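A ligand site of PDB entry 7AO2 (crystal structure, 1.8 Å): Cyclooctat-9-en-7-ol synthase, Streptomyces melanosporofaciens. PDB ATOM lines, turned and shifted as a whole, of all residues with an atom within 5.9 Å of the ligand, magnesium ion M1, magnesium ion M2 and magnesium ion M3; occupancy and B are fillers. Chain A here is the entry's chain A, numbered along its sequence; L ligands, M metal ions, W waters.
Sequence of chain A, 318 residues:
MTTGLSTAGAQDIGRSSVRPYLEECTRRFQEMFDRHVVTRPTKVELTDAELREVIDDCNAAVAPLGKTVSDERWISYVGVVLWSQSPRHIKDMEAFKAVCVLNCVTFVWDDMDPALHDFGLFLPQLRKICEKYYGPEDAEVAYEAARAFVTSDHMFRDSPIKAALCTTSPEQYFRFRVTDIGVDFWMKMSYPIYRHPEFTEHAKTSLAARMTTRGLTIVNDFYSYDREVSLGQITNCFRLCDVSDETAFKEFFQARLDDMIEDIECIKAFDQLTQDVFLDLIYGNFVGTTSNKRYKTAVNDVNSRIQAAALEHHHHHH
OH of Tyr 295 is in hydrogen-bond range of O1 of the ligand (2.5 Å).
NH1 of Arg 177 is in salt-bridge range of O6 of the ligand, at 2.7 Å.
The guanidinium group (NH2) of Arg 227 is in salt-bridge range of an oxygen (O1) of the ligand (3.4 Å).
O1 of the ligand is in salt-bridge range of NE of Arg 294.
The backbone carbonyl oxygen of Ile 181 lies within hydrogen-bond range of a nitrogen (N1) of the ligand, 2.9 Å away.
NH1 of Arg 227 lies close to OE2 of Glu 228, 3.9 Å away.
O of Glu 228 sits at hydrogen-bond distance from N of Gln 233, 2.9 Å away.
NH2 of Arg 177 is in salt-bridge range of OD1 of Asp 221 (2.9 Å).
The side-chain carboxylate of Glu 228 is in hydrogen-bond range of the side-chain amide nitrogen of Asn 236.
NH1 of Arg 177 is in salt-bridge range of OD2 of Asp 180, 2.9 Å away.
The guanidinium group of Arg 294 lies within salt-bridge range of the side-chain carboxylate of Asp 111 (2.7 Å).
The side-chain amide nitrogen (ND2) of Asn 220 lies close to the side-chain hydroxyl (OH) of Tyr 295 (3.4 Å).
Residues that only touch the ligand: Phe 107 (3.5 Å).
Hydrophobic or aromatic side chains that line the ligand: Phe 107, Ile 181 and Tyr 295.
One residue has an atom within 4 Å of magnesium ion M1: Asp 110.
Of the 22 residues printed, 3 come within 4 Å of magnesium ion M2.
One residue has an atom within 4 Å of magnesium ion M3: Asp 110.
The nearest printed residue that does not touch magnesium ion M3 is Asp 180 (4.1 Å).
OD2 of Asp 110 is bound to magnesium ion M1 (2.0 Å).
An oxygen (O3) of the ligand binds magnesium ion M1, 2.1 Å away.
Water W5 is bound to magnesium ion M1 (2.1 Å).
Magnesium ion M1 is bound by water W3 (2.1 Å).
Magnesium ion M1 is bound by an oxygen (O4) of the ligand (2.1 Å).
Magnesium ion M1 is bound by water W7, at 2.4 Å.
An oxygen (O2) of the ligand is bound to magnesium ion M2, at 2.0 Å.
The side-chain carboxylate (OE2) of Glu 228 is bound to magnesium ion M2.
Magnesium ion M2 is bound by O5 of the ligand, at 2.1 Å.
Magnesium ion M2 is bound by OD1 of Asn 220 (2.2 Å).
Magnesium ion M2 is bound by water W8, 2.2 Å away.
Magnesium ion M2 is bound by OG of Ser 224 (2.3 Å).
Magnesium ion M3 is bound by OD1 of Asp 110, water W1, water W6, O4 of the ligand, water W4 and water W7.
Magnesium ion M3 has six donor atoms within binding distance.
Water W4 lies within hydrogen-bond range of OD1 of Asp 153 (2.7 Å) and OD1 of Asp 180 (3.0 Å).
Water W1 lies within hydrogen-bond range of O6 of the ligand and O of Asp 180.
Water W6 bridges the side-chain carboxylate (OD2) of Asp 180 and the guanidinium group (NH1) of Arg 177.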
ATOM      1  N   ASN A 103     -24.314 -11.454  16.104  1.00  0.00           N
ATOM      2  CA  ASN A 103     -24.136 -11.120  17.528  1.00  0.00           C
ATOM      3  C   ASN A 103     -25.353 -11.520  18.341  1.00  0.00           C
ATOM      4  O   ASN A 103     -25.225 -12.171  19.388  1.00  0.00           O
ATOM      5  CB  ASN A 103     -23.861  -9.609  17.689  1.00  0.00           C
ATOM      6  CG  ASN A 103     -23.874  -9.153  19.141  1.00  0.00           C
ATOM      7  OD1 ASN A 103     -22.816  -9.198  19.812  1.00  0.00           O
ATOM      8  ND2 ASN A 103     -25.047  -8.655  19.641  1.00  0.00           N
ATOM      9  N   THR A 106     -26.081 -15.396  18.635  1.00  0.00           N
ATOM     10  CA  THR A 106     -25.126 -16.148  19.445  1.00  0.00           C
ATOM     11  C   THR A 106     -25.132 -15.699  20.896  1.00  0.00           C
ATOM     12  O   THR A 106     -24.689 -16.445  21.768  1.00  0.00           O
ATOM     13  CB  THR A 106     -23.709 -16.085  18.861  1.00  0.00           C
ATOM     14  OG1 THR A 106     -23.262 -14.723  18.777  1.00  0.00           O
ATOM     15  CG2 THR A 106     -23.707 -16.704  17.479  1.00  0.00           C
ATOM     16  N   PHE A 107     -25.658 -14.498  21.178  1.00  0.00           N
ATOM     17  CA  PHE A 107     -25.962 -14.149  22.560  1.00  0.00           C
ATOM     18  C   PHE A 107     -27.017 -15.085  23.141  1.00  0.00           C
ATOM     19  O   PHE A 107     -26.939 -15.467  24.311  1.00  0.00           O
ATOM     20  CB  PHE A 107     -26.480 -12.709  22.626  1.00  0.00           C
ATOM     21  CG  PHE A 107     -25.531 -11.715  23.223  1.00  0.00           C
ATOM     22  CD1 PHE A 107     -25.340 -11.636  24.608  1.00  0.00           C
ATOM     23  CD2 PHE A 107     -24.866 -10.802  22.401  1.00  0.00           C
ATOM     24  CE1 PHE A 107     -24.517 -10.674  25.176  1.00  0.00           C
ATOM     25  CE2 PHE A 107     -23.985  -9.840  22.962  1.00  0.00           C
ATOM     26  CZ  PHE A 107     -23.818  -9.771  24.364  1.00  0.00           C
ATOM     27  N   ASP A 110     -25.239 -18.125  24.105  1.00  0.00           N
ATOM     28  CA  ASP A 110     -24.458 -17.894  25.315  1.00  0.00           C
ATOM     29  C   ASP A 110     -25.342 -18.001  26.557  1.00  0.00           C
ATOM     30  O   ASP A 110     -24.912 -18.502  27.603  1.00  0.00           O
ATOM     31  CB  ASP A 110     -23.819 -16.493  25.211  1.00  0.00           C
ATOM     32  CG  ASP A 110     -22.872 -16.149  26.361  1.00  0.00           C
ATOM     33  OD1 ASP A 110     -21.726 -16.608  26.277  1.00  0.00           O
ATOM     34  OD2 ASP A 110     -23.228 -15.357  27.311  1.00  0.00           O
ATOM     35  N   ASP A 111     -26.578 -17.553  26.453  1.00  0.00           N
ATOM     36  CA  ASP A 111     -27.470 -17.552  27.597  1.00  0.00           C
ATOM     37  C   ASP A 111     -28.188 -18.884  27.799  1.00  0.00           C
ATOM     38  O   ASP A 111     -28.884 -19.033  28.817  1.00  0.00           O
ATOM     39  CB  ASP A 111     -28.509 -16.425  27.412  1.00  0.00           C
ATOM     40  CG  ASP A 111     -27.956 -15.059  27.820  1.00  0.00           C
ATOM     41  OD1 ASP A 111     -26.941 -15.026  28.543  1.00  0.00           O
ATOM     42  OD2 ASP A 111     -28.513 -14.020  27.394  1.00  0.00           O
ATOM     43  N   PHE A 149     -17.300 -19.929  17.430  1.00  0.00           N
ATOM     44  CA  PHE A 149     -17.747 -19.309  18.685  1.00  0.00           C
ATOM     45  C   PHE A 149     -18.771 -20.175  19.414  1.00  0.00           C
ATOM     46  O   PHE A 149     -18.653 -20.378  20.636  1.00  0.00           O
ATOM     47  CB  PHE A 149     -18.334 -17.907  18.432  1.00  0.00           C
ATOM     48  CG  PHE A 149     -18.932 -17.314  19.693  1.00  0.00           C
ATOM     49  CD1 PHE A 149     -18.124 -16.676  20.634  1.00  0.00           C
ATOM     50  CD2 PHE A 149     -20.303 -17.447  19.958  1.00  0.00           C
ATOM     51  CE1 PHE A 149     -18.670 -16.128  21.850  1.00  0.00           C
ATOM     52  CE2 PHE A 149     -20.868 -16.926  21.123  1.00  0.00           C
ATOM     53  CZ  PHE A 149     -20.054 -16.270  22.089  1.00  0.00           C
ATOM     54  N   ASP A 153     -18.256 -22.042  23.143  1.00  0.00           N
ATOM     55  CA  ASP A 153     -19.110 -21.847  24.299  1.00  0.00           C
ATOM     56  C   ASP A 153     -19.693 -23.173  24.786  1.00  0.00           C
ATOM     57  O   ASP A 153     -19.802 -23.416  25.988  1.00  0.00           O
ATOM     58  CB  ASP A 153     -20.213 -20.869  23.919  1.00  0.00           C
ATOM     59  CG  ASP A 153     -21.216 -20.735  25.010  1.00  0.00           C
ATOM     60  OD1 ASP A 153     -20.843 -20.338  26.128  1.00  0.00           O
ATOM     61  OD2 ASP A 153     -22.386 -21.023  24.741  1.00  0.00           O
ATOM     62  N   ARG A 177     -10.225 -15.861  26.738  1.00  0.00           N
ATOM     63  CA  ARG A 177     -11.287 -14.954  26.364  1.00  0.00           C
ATOM     64  C   ARG A 177     -11.155 -14.431  24.934  1.00  0.00           C
ATOM     65  O   ARG A 177     -12.153 -13.979  24.382  1.00  0.00           O
ATOM     66  CB  ARG A 177     -11.335 -13.797  27.369  1.00  0.00           C
ATOM     67  CG  ARG A 177     -11.892 -14.238  28.726  1.00  0.00           C
ATOM     68  CD  ARG A 177     -13.378 -14.676  28.645  1.00  0.00           C
ATOM     69  NE  ARG A 177     -14.189 -13.667  29.341  1.00  0.00           N
ATOM     70  CZ  ARG A 177     -15.447 -13.386  29.052  1.00  0.00           C
ATOM     71  NH1 ARG A 177     -16.097 -14.043  28.083  1.00  0.00           N
ATOM     72  NH2 ARG A 177     -16.062 -12.429  29.727  1.00  0.00           N
ATOM     73  N   ASP A 180     -13.465 -16.783  23.702  1.00  0.00           N
ATOM     74  CA  ASP A 180     -14.714 -17.070  24.417  1.00  0.00           C
ATOM     75  C   ASP A 180     -15.615 -15.840  24.513  1.00  0.00           C
ATOM     76  O   ASP A 180     -16.840 -15.950  24.431  1.00  0.00           O
ATOM     77  CB  ASP A 180     -14.408 -17.602  25.826  1.00  0.00           C
ATOM     78  CG  ASP A 180     -15.673 -17.791  26.665  1.00  0.00           C
ATOM     79  OD1 ASP A 180     -16.362 -18.826  26.498  1.00  0.00           O
ATOM     80  OD2 ASP A 180     -15.986 -16.896  27.481  1.00  0.00           O
ATOM     81  N   ILE A 181     -15.029 -14.656  24.688  1.00  0.00           N
ATOM     82  CA  ILE A 181     -15.903 -13.481  24.756  1.00  0.00           C
ATOM     83  C   ILE A 181     -16.459 -13.135  23.384  1.00  0.00           C
ATOM     84  O   ILE A 181     -17.417 -12.344  23.276  1.00  0.00           O
ATOM     85  CB  ILE A 181     -15.148 -12.285  25.352  1.00  0.00           C
ATOM     86  CG1 ILE A 181     -16.173 -11.225  25.866  1.00  0.00           C
ATOM     87  CG2 ILE A 181     -14.144 -11.656  24.309  1.00  0.00           C
ATOM     88  CD1 ILE A 181     -15.576 -10.138  26.741  1.00  0.00           C
ATOM     89  N   GLY A 182     -15.869 -13.681  22.311  1.00  0.00           N
ATOM     90  CA  GLY A 182     -16.441 -13.502  21.000  1.00  0.00           C
ATOM     91  C   GLY A 182     -15.788 -12.423  20.179  1.00  0.00           C
ATOM     92  O   GLY A 182     -16.271 -12.126  19.074  1.00  0.00           O
ATOM     93  N   ASN A 220     -16.562  -5.857  30.428  1.00  0.00           N
ATOM     94  CA  ASN A 220     -17.671  -6.792  30.547  1.00  0.00           C
ATOM     95  C   ASN A 220     -17.645  -7.543  31.889  1.00  0.00           C
ATOM     96  O   ASN A 220     -18.680  -7.700  32.537  1.00  0.00           O
ATOM     97  CB  ASN A 220     -17.684  -7.807  29.423  1.00  0.00           C
ATOM     98  CG  ASN A 220     -18.798  -8.821  29.635  1.00  0.00           C
ATOM     99  OD1 ASN A 220     -18.547  -9.897  30.104  1.00  0.00           O
ATOM    100  ND2 ASN A 220     -20.044  -8.401  29.416  1.00  0.00           N
ATOM    101  N   ASP A 221     -16.476  -8.009  32.321  1.00  0.00           N
ATOM    102  CA  ASP A 221     -16.418  -8.764  33.564  1.00  0.00           C
ATOM    103  C   ASP A 221     -16.912  -7.954  34.770  1.00  0.00           C
ATOM    104  O   ASP A 221     -17.606  -8.482  35.659  1.00  0.00           O
ATOM    105  CB  ASP A 221     -14.992  -9.253  33.799  1.00  0.00           C
ATOM    106  CG  ASP A 221     -14.575 -10.352  32.842  1.00  0.00           C
ATOM    107  OD1 ASP A 221     -15.446 -10.832  32.075  1.00  0.00           O
ATOM    108  OD2 ASP A 221     -13.395 -10.723  32.874  1.00  0.00           O
ATOM    109  N   SER A 224     -20.810  -7.727  34.504  1.00  0.00           N
ATOM    110  CA  SER A 224     -21.570  -8.986  34.496  1.00  0.00           C
ATOM    111  C   SER A 224     -21.194  -9.896  35.670  1.00  0.00           C
ATOM    112  O   SER A 224     -21.742 -11.000  35.790  1.00  0.00           O
ATOM    113  CB  SER A 224     -21.409  -9.721  33.148  1.00  0.00           C
ATOM    114  OG  SER A 224     -20.041  -9.921  32.800  1.00  0.00           O
ATOM    115  N   TYR A 225     -20.311  -9.428  36.567  1.00  0.00           N
ATOM    116  CA  TYR A 225     -19.863 -10.243  37.702  1.00  0.00           C
ATOM    117  C   TYR A 225     -21.037 -10.729  38.562  1.00  0.00           C
ATOM    118  O   TYR A 225     -21.110 -11.923  38.911  1.00  0.00           O
ATOM    119  CB  TYR A 225     -18.904  -9.423  38.564  1.00  0.00           C
ATOM    120  CG  TYR A 225     -18.354 -10.179  39.766  1.00  0.00           C
ATOM    121  CD1 TYR A 225     -17.178 -10.918  39.656  1.00  0.00           C
ATOM    122  CD2 TYR A 225     -18.992 -10.133  41.022  1.00  0.00           C
ATOM    123  CE1 TYR A 225     -16.652 -11.619  40.742  1.00  0.00           C
ATOM    124  CE2 TYR A 225     -18.464 -10.849  42.149  1.00  0.00           C
ATOM    125  CZ  TYR A 225     -17.291 -11.587  41.981  1.00  0.00           C
ATOM    126  OH  TYR A 225     -16.711 -12.289  43.015  1.00  0.00           O
ATOM    127  N   ARG A 227     -24.269 -11.112  38.068  1.00  0.00           N
ATOM    128  CA  ARG A 227     -25.050 -12.135  37.371  1.00  0.00           C
ATOM    129  C   ARG A 227     -24.274 -13.449  37.265  1.00  0.00           C
ATOM    130  O   ARG A 227     -24.796 -14.545  37.571  1.00  0.00           O
ATOM    131  CB  ARG A 227     -25.469 -11.651  35.968  1.00  0.00           C
ATOM    132  CG  ARG A 227     -25.772 -12.803  35.001  1.00  0.00           C
ATOM    133  CD  ARG A 227     -26.445 -12.407  33.717  1.00  0.00           C
ATOM    134  NE  ARG A 227     -25.762 -11.326  33.023  1.00  0.00           N
ATOM    135  CZ  ARG A 227     -24.793 -11.505  32.123  1.00  0.00           C
ATOM    136  NH1 ARG A 227     -24.421 -12.746  31.793  1.00  0.00           N
ATOM    137  NH2 ARG A 227     -24.226 -10.454  31.525  1.00  0.00           N
ATOM    138  N   GLU A 228     -23.029 -13.389  36.820  1.00  0.00           N
ATOM    139  CA  GLU A 228     -22.292 -14.619  36.558  1.00  0.00           C
ATOM    140  C   GLU A 228     -22.017 -15.385  37.848  1.00  0.00           C
ATOM    141  O   GLU A 228     -22.235 -16.607  37.913  1.00  0.00           O
ATOM    142  CB  GLU A 228     -21.003 -14.306  35.788  1.00  0.00           C
ATOM    143  CG  GLU A 228     -21.372 -13.922  34.351  1.00  0.00           C
ATOM    144  CD  GLU A 228     -20.255 -13.225  33.581  1.00  0.00           C
ATOM    145  OE1 GLU A 228     -19.122 -13.125  34.121  1.00  0.00           O
ATOM    146  OE2 GLU A 228     -20.525 -12.829  32.434  1.00  0.00           O
ATOM    147  N   GLN A 233     -21.120 -19.202  37.068  1.00  0.00           N
ATOM    148  CA  GLN A 233     -20.271 -19.011  35.896  1.00  0.00           C
ATOM    149  C   GLN A 233     -18.890 -18.492  36.334  1.00  0.00           C
ATOM    150  O   GLN A 233     -18.776 -17.503  37.046  1.00  0.00           O
ATOM    151  CB  GLN A 233     -20.980 -18.053  34.937  1.00  0.00           C
ATOM    152  CG  GLN A 233     -22.177 -18.766  34.275  1.00  0.00           C
ATOM    153  CD  GLN A 233     -22.960 -17.827  33.398  1.00  0.00           C
ATOM    154  OE1 GLN A 233     -23.255 -16.711  33.808  1.00  0.00           O
ATOM    155  NE2 GLN A 233     -23.273 -18.255  32.165  1.00  0.00           N
ATOM    156  N   THR A 235     -16.210 -17.698  34.294  1.00  0.00           N
ATOM    157  CA  THR A 235     -15.420 -16.980  33.292  1.00  0.00           C
ATOM    158  C   THR A 235     -15.536 -15.479  33.578  1.00  0.00           C
ATOM    159  O   THR A 235     -16.266 -14.724  32.912  1.00  0.00           O
ATOM    160  CB  THR A 235     -15.889 -17.347  31.878  1.00  0.00           C
ATOM    161  OG1 THR A 235     -15.910 -18.780  31.733  1.00  0.00           O
ATOM    162  CG2 THR A 235     -14.975 -16.754  30.788  1.00  0.00           C
ATOM    163  N   ASN A 236     -14.759 -15.020  34.569  1.00  0.00           N
ATOM    164  CA  ASN A 236     -14.806 -13.599  34.957  1.00  0.00           C
ATOM    165  C   ASN A 236     -13.520 -13.271  35.711  1.00  0.00           C
ATOM    166  O   ASN A 236     -13.248 -13.887  36.752  1.00  0.00           O
ATOM    167  CB  ASN A 236     -16.029 -13.334  35.814  1.00  0.00           C
ATOM    168  CG  ASN A 236     -16.228 -11.852  36.079  1.00  0.00           C
ATOM    169  OD1 ASN A 236     -15.323 -11.173  36.583  1.00  0.00           O
ATOM    170  ND2 ASN A 236     -17.423 -11.321  35.706  1.00  0.00           N
ATOM    171  N   ARG A 294     -29.143  -5.275  30.525  1.00  0.00           N
ATOM    172  CA  ARG A 294     -28.492  -6.553  30.780  1.00  0.00           C
ATOM    173  C   ARG A 294     -27.459  -6.453  31.909  1.00  0.00           C
ATOM    174  O   ARG A 294     -27.246  -7.422  32.654  1.00  0.00           O
ATOM    175  CB  ARG A 294     -27.841  -7.055  29.491  1.00  0.00           C
ATOM    176  CG  ARG A 294     -27.017  -8.350  29.699  1.00  0.00           C
ATOM    177  CD  ARG A 294     -26.575  -8.900  28.347  1.00  0.00           C
ATOM    178  NE  ARG A 294     -25.894 -10.208  28.456  1.00  0.00           N
ATOM    179  CZ  ARG A 294     -26.504 -11.399  28.450  1.00  0.00           C
ATOM    180  NH1 ARG A 294     -27.825 -11.488  28.374  1.00  0.00           N
ATOM    181  NH2 ARG A 294     -25.792 -12.528  28.509  1.00  0.00           N
ATOM    182  N   TYR A 295     -26.795  -5.319  32.063  1.00  0.00           N
ATOM    183  CA  TYR A 295     -25.616  -5.243  32.923  1.00  0.00           C
ATOM    184  C   TYR A 295     -25.879  -4.417  34.181  1.00  0.00           C
ATOM    185  O   TYR A 295     -25.023  -3.632  34.634  1.00  0.00           O
ATOM    186  CB  TYR A 295     -24.431  -4.725  32.128  1.00  0.00           C
ATOM    187  CG  TYR A 295     -24.100  -5.604  30.962  1.00  0.00           C
ATOM    188  CD1 TYR A 295     -23.584  -6.893  31.184  1.00  0.00           C
ATOM    189  CD2 TYR A 295     -24.240  -5.159  29.644  1.00  0.00           C
ATOM    190  CE1 TYR A 295     -23.261  -7.735  30.140  1.00  0.00           C
ATOM    191  CE2 TYR A 295     -23.926  -5.991  28.565  1.00  0.00           C
ATOM    192  CZ  TYR A 295     -23.417  -7.277  28.837  1.00  0.00           C
ATOM    193  OH  TYR A 295     -23.089  -8.118  27.838  1.00  0.00           O
HETATM  194  C1  LIG L   1     -20.609 -12.317  25.094  1.00  0.00           C
HETATM  195  C2  LIG L   1     -21.277 -12.352  23.703  1.00  0.00           C
HETATM  196  C3  LIG L   1     -21.606 -12.362  26.312  1.00  0.00           C
HETATM  197  C4  LIG L   1     -20.878 -11.888  27.596  1.00  0.00           C
HETATM  198  O1  LIG L   1     -23.105 -10.512  28.363  1.00  0.00           O
HETATM  199  P1  LIG L   1     -22.121 -11.527  28.903  1.00  0.00           P
HETATM  200  O2  LIG L   1     -21.491 -11.033  30.172  1.00  0.00           O
HETATM  201  O3  LIG L   1     -22.807 -12.838  29.199  1.00  0.00           O
HETATM  202  P2  LIG L   1     -19.692 -13.159  28.215  1.00  0.00           P
HETATM  203  O4  LIG L   1     -20.434 -14.498  28.253  1.00  0.00           O
HETATM  204  O5  LIG L   1     -19.240 -12.819  29.601  1.00  0.00           O
HETATM  205  O6  LIG L   1     -18.543 -13.262  27.191  1.00  0.00           O
HETATM  206  O7  LIG L   1     -20.110 -10.729  27.412  1.00  0.00           O
HETATM  207  N1  LIG L   1     -20.251 -12.147  22.670  1.00  0.00           N
HETATM  208 MG    MG M   1     -22.380 -14.852  29.059  1.00  0.00          MG
HETATM  209 MG    MG M   2     -19.735 -11.443  31.135  1.00  0.00          MG
HETATM  210 MG    MG M   3     -20.036 -16.372  27.346  1.00  0.00          MG
HETATM  211  O   HOH W   1     -19.053 -15.376  25.825  1.00  0.00           O
HETATM  212  O   HOH W   2     -18.233 -15.003  30.919  1.00  0.00           O
HETATM  213  O   HOH W   3     -24.223 -15.625  29.712  1.00  0.00           O
HETATM  214  O   HOH W   4     -19.273 -18.247  26.678  1.00  0.00           O
HETATM  215  O   HOH W   5     -21.866 -14.868  31.088  1.00  0.00           O
HETATM  216  O   HOH W   6     -18.380 -16.481  28.650  1.00  0.00           O
HETATM  217  O   HOH W   7     -21.288 -16.991  29.027  1.00  0.00           O
HETATM  218  O   HOH W   8     -17.775 -11.820  32.123  1.00  0.00           O
